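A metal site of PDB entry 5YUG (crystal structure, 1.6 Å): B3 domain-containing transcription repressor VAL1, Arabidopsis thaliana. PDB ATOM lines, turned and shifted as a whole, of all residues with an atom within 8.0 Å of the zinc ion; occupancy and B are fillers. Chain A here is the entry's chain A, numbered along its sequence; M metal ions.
Four residues have an atom within 4 Å of the zinc ion: Cys 65, Cys 68, Cys 93 and Cys 96.
The nearest printed residue that does not touch the zinc ion is Lys 70 (4.6 Å).
The side-chain sulfur (SG) of Cys 96 binds the zinc ion.
SG of Cys 68 binds the zinc ion, at 2.3 Å.
The zinc ion is bound by SG of Cys 65 (2.4 Å).
The zinc ion is bound by SG of Cys 93 (2.4 Å).
The backbone carbonyl oxygen (O) of Cys 96 is in hydrogen-bond range of the side-chain hydroxyl (OH) of Tyr 66 (3.4 Å).
N of Lys 70 sits close to SG of Cys 68, at 3.4 Å.
O of Lys 70 lies within hydrogen-bond range of N of Cys 65, 2.8 Å away.
The backbone NH (N) of Leu 67 sits close to the side-chain sulfur (SG) of Cys 65, at 3.5 Å.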
ATOM      1  N   GLU A  64     -22.932  25.143 -24.506  1.00  0.00           N
ATOM      2  CA  GLU A  64     -24.016  25.609 -23.644  1.00  0.00           C
ATOM      3  C   GLU A  64     -24.525  24.475 -22.746  1.00  0.00           C
ATOM      4  O   GLU A  64     -24.695  23.343 -23.204  1.00  0.00           O
ATOM      5  CB  GLU A  64     -25.168  26.154 -24.479  1.00  0.00           C
ATOM      6  CG  GLU A  64     -24.838  27.501 -25.139  1.00  0.00           C
ATOM      7  CD  GLU A  64     -25.907  27.954 -26.120  1.00  0.00           C
ATOM      8  OE1 GLU A  64     -26.978  27.304 -26.191  1.00  0.00           O
ATOM      9  OE2 GLU A  64     -25.680  28.965 -26.809  1.00  0.00           O
ATOM     10  N   CYS A  65     -24.762  24.804 -21.480  1.00  0.00           N
ATOM     11  CA  CYS A  65     -25.407  23.847 -20.577  1.00  0.00           C
ATOM     12  C   CYS A  65     -26.725  23.348 -21.167  1.00  0.00           C
ATOM     13  O   CYS A  65     -27.541  24.141 -21.659  1.00  0.00           O
ATOM     14  CB  CYS A  65     -25.649  24.518 -19.222  1.00  0.00           C
ATOM     15  SG  CYS A  65     -26.536  23.483 -18.033  1.00  0.00           S
ATOM     16  N   TYR A  66     -26.938  22.029 -21.099  1.00  0.00           N
ATOM     17  CA  TYR A  66     -28.152  21.438 -21.658  1.00  0.00           C
ATOM     18  C   TYR A  66     -29.439  21.909 -20.974  1.00  0.00           C
ATOM     19  O   TYR A  66     -30.515  21.798 -21.580  1.00  0.00           O
ATOM     20  CB  TYR A  66     -28.076  19.905 -21.560  1.00  0.00           C
ATOM     21  CG  TYR A  66     -28.427  19.380 -20.197  1.00  0.00           C
ATOM     22  CD1 TYR A  66     -27.547  19.528 -19.137  1.00  0.00           C
ATOM     23  CD2 TYR A  66     -29.649  18.775 -19.961  1.00  0.00           C
ATOM     24  CE1 TYR A  66     -27.861  19.072 -17.885  1.00  0.00           C
ATOM     25  CE2 TYR A  66     -29.981  18.309 -18.699  1.00  0.00           C
ATOM     26  CZ  TYR A  66     -29.083  18.457 -17.669  1.00  0.00           C
ATOM     27  OH  TYR A  66     -29.385  17.989 -16.417  1.00  0.00           O
ATOM     28  N   LEU A  67     -29.338  22.425 -19.750  1.00  0.00           N
ATOM     29  CA  LEU A  67     -30.502  22.795 -18.956  1.00  0.00           C
ATOM     30  C   LEU A  67     -30.732  24.298 -18.909  1.00  0.00           C
ATOM     31  O   LEU A  67     -31.833  24.755 -19.217  1.00  0.00           O
ATOM     32  CB  LEU A  67     -30.361  22.245 -17.530  1.00  0.00           C
ATOM     33  CG  LEU A  67     -31.581  22.435 -16.617  1.00  0.00           C
ATOM     34  CD1 LEU A  67     -32.779  21.628 -17.116  1.00  0.00           C
ATOM     35  CD2 LEU A  67     -31.230  22.072 -15.188  1.00  0.00           C
ATOM     36  N   CYS A  68     -29.708  25.084 -18.551  1.00  0.00           N
ATOM     37  CA  CYS A  68     -29.864  26.525 -18.403  1.00  0.00           C
ATOM     38  C   CYS A  68     -29.211  27.333 -19.503  1.00  0.00           C
ATOM     39  O   CYS A  68     -29.419  28.553 -19.567  1.00  0.00           O
ATOM     40  CB  CYS A  68     -29.318  26.985 -17.038  1.00  0.00           C
ATOM     41  SG  CYS A  68     -27.506  27.065 -16.981  1.00  0.00           S
ATOM     42  N   SER A  69     -28.405  26.702 -20.372  1.00  0.00           N
ATOM     43  CA  SER A  69     -27.752  27.315 -21.535  1.00  0.00           C
ATOM     44  C   SER A  69     -26.596  28.225 -21.152  1.00  0.00           C
ATOM     45  O   SER A  69     -26.096  28.938 -22.028  1.00  0.00           O
ATOM     46  CB  SER A  69     -28.721  28.103 -22.421  1.00  0.00           C
ATOM     47  OG  SER A  69     -29.802  27.303 -22.866  1.00  0.00           O
ATOM     48  N   LYS A  70     -26.166  28.216 -19.893  1.00  0.00           N
ATOM     49  CA  LYS A  70     -24.955  28.939 -19.528  1.00  0.00           C
ATOM     50  C   LYS A  70     -23.816  28.523 -20.443  1.00  0.00           C
ATOM     51  O   LYS A  70     -23.691  27.343 -20.805  1.00  0.00           O
ATOM     52  CB  LYS A  70     -24.565  28.652 -18.075  1.00  0.00           C
ATOM     53  CG  LYS A  70     -23.434  29.538 -17.587  1.00  0.00           C
ATOM     54  CD  LYS A  70     -23.055  29.170 -16.195  1.00  0.00           C
ATOM     55  CE  LYS A  70     -21.985  30.055 -15.603  1.00  0.00           C
ATOM     56  NZ  LYS A  70     -21.850  29.767 -14.150  1.00  0.00           N
ATOM     57  N   ARG A  71     -22.974  29.486 -20.820  1.00  0.00           N
ATOM     58  CA  ARG A  71     -21.836  29.171 -21.668  1.00  0.00           C
ATOM     59  C   ARG A  71     -20.705  28.655 -20.791  1.00  0.00           C
ATOM     60  O   ARG A  71     -20.348  29.264 -19.793  1.00  0.00           O
ATOM     61  CB  ARG A  71     -21.405  30.394 -22.463  1.00  0.00           C
ATOM     62  CG  ARG A  71     -22.332  30.654 -23.619  1.00  0.00           C
ATOM     63  CD  ARG A  71     -21.706  30.095 -24.918  1.00  0.00           C
ATOM     64  NE  ARG A  71     -20.766  31.022 -25.491  1.00  0.00           N
ATOM     65  CZ  ARG A  71     -20.182  30.809 -26.664  1.00  0.00           C
ATOM     66  NH1 ARG A  71     -20.443  29.700 -27.353  1.00  0.00           N
ATOM     67  NH2 ARG A  71     -19.325  31.676 -27.159  1.00  0.00           N
ATOM     68  N   LEU A  72     -20.195  27.486 -21.165  1.00  0.00           N
ATOM     69  CA  LEU A  72     -19.249  26.713 -20.379  1.00  0.00           C
ATOM     70  C   LEU A  72     -18.006  26.483 -21.239  1.00  0.00           C
ATOM     71  O   LEU A  72     -18.107  25.922 -22.343  1.00  0.00           O
ATOM     72  CB  LEU A  72     -19.884  25.381 -19.968  1.00  0.00           C
ATOM     73  CG  LEU A  72     -21.164  25.414 -19.124  1.00  0.00           C
ATOM     74  CD1 LEU A  72     -21.704  23.989 -18.953  1.00  0.00           C
ATOM     75  CD2 LEU A  72     -20.874  25.999 -17.739  1.00  0.00           C
ATOM     76  N   THR A  82     -16.403  23.204 -12.834  1.00  0.00           N
ATOM     77  CA  THR A  82     -17.821  23.563 -12.918  1.00  0.00           C
ATOM     78  C   THR A  82     -18.599  22.851 -14.020  1.00  0.00           C
ATOM     79  O   THR A  82     -19.803  23.131 -14.169  1.00  0.00           O
ATOM     80  CB  THR A  82     -17.987  25.082 -13.121  1.00  0.00           C
ATOM     81  OG1 THR A  82     -17.435  25.469 -14.384  1.00  0.00           O
ATOM     82  CG2 THR A  82     -17.311  25.846 -12.017  1.00  0.00           C
ATOM     83  N   VAL A  91     -22.771  18.890 -22.187  1.00  0.00           N
ATOM     84  CA  VAL A  91     -22.347  19.280 -20.847  1.00  0.00           C
ATOM     85  C   VAL A  91     -23.503  19.908 -20.098  1.00  0.00           C
ATOM     86  O   VAL A  91     -24.468  20.416 -20.673  1.00  0.00           O
ATOM     87  CB  VAL A  91     -21.155  20.254 -20.889  1.00  0.00           C
ATOM     88  CG1 VAL A  91     -19.913  19.542 -21.363  1.00  0.00           C
ATOM     89  CG2 VAL A  91     -21.469  21.442 -21.834  1.00  0.00           C
ATOM     90  N   GLY A  92     -23.361  19.884 -18.778  1.00  0.00           N
ATOM     91  CA  GLY A  92     -24.210  20.679 -17.911  1.00  0.00           C
ATOM     92  C   GLY A  92     -23.363  21.336 -16.843  1.00  0.00           C
ATOM     93  O   GLY A  92     -22.276  20.857 -16.511  1.00  0.00           O
ATOM     94  N   CYS A  93     -23.845  22.472 -16.347  1.00  0.00           N
ATOM     95  CA  CYS A  93     -23.303  22.999 -15.096  1.00  0.00           C
ATOM     96  C   CYS A  93     -23.283  21.907 -14.053  1.00  0.00           C
ATOM     97  O   CYS A  93     -24.217  21.096 -13.987  1.00  0.00           O
ATOM     98  CB  CYS A  93     -24.166  24.152 -14.606  1.00  0.00           C
ATOM     99  SG  CYS A  93     -24.355  25.482 -15.757  1.00  0.00           S
ATOM    100  N   SER A  94     -22.249  21.883 -13.206  1.00  0.00           N
ATOM    101  CA  SER A  94     -22.258  20.922 -12.105  1.00  0.00           C
ATOM    102  C   SER A  94     -23.541  21.016 -11.289  1.00  0.00           C
ATOM    103  O   SER A  94     -24.111  19.987 -10.877  1.00  0.00           O
ATOM    104  CB  SER A  94     -21.030  21.153 -11.197  1.00  0.00           C
ATOM    105  OG  SER A  94     -19.833  20.871 -11.904  1.00  0.00           O
ATOM    106  N   THR A  95     -24.061  22.226 -11.127  1.00  0.00           N
ATOM    107  CA  THR A  95     -25.250  22.461 -10.329  1.00  0.00           C
ATOM    108  C   THR A  95     -26.551  22.208 -11.093  1.00  0.00           C
ATOM    109  O   THR A  95     -27.621  22.202 -10.476  1.00  0.00           O
ATOM    110  CB  THR A  95     -25.207  23.881  -9.780  1.00  0.00           C
ATOM    111  OG1 THR A  95     -24.993  24.791 -10.871  1.00  0.00           O
ATOM    112  CG2 THR A  95     -24.031  24.036  -8.816  1.00  0.00           C
ATOM    113  N   CYS A  96     -26.481  22.028 -12.420  1.00  0.00           N
ATOM    114  CA  CYS A  96     -27.630  21.648 -13.231  1.00  0.00           C
ATOM    115  C   CYS A  96     -27.701  20.135 -13.431  1.00  0.00           C
ATOM    116  O   CYS A  96     -28.782  19.544 -13.400  1.00  0.00           O
ATOM    117  CB  CYS A  96     -27.562  22.310 -14.609  1.00  0.00           C
ATOM    118  SG  CYS A  96     -27.894  24.074 -14.578  1.00  0.00           S
ATOM    119  N   ALA A  97     -26.531  19.522 -13.639  1.00  0.00           N
ATOM    120  CA  ALA A  97     -26.443  18.149 -14.118  1.00  0.00           C
ATOM    121  C   ALA A  97     -26.987  17.142 -13.125  1.00  0.00           C
ATOM    122  O   ALA A  97     -27.380  16.029 -13.524  1.00  0.00           O
ATOM    123  CB  ALA A  97     -24.993  17.810 -14.468  1.00  0.00           C
HETATM  124 ZN    ZN M   1     -26.697  25.032 -16.269  1.00  0.00          ZN
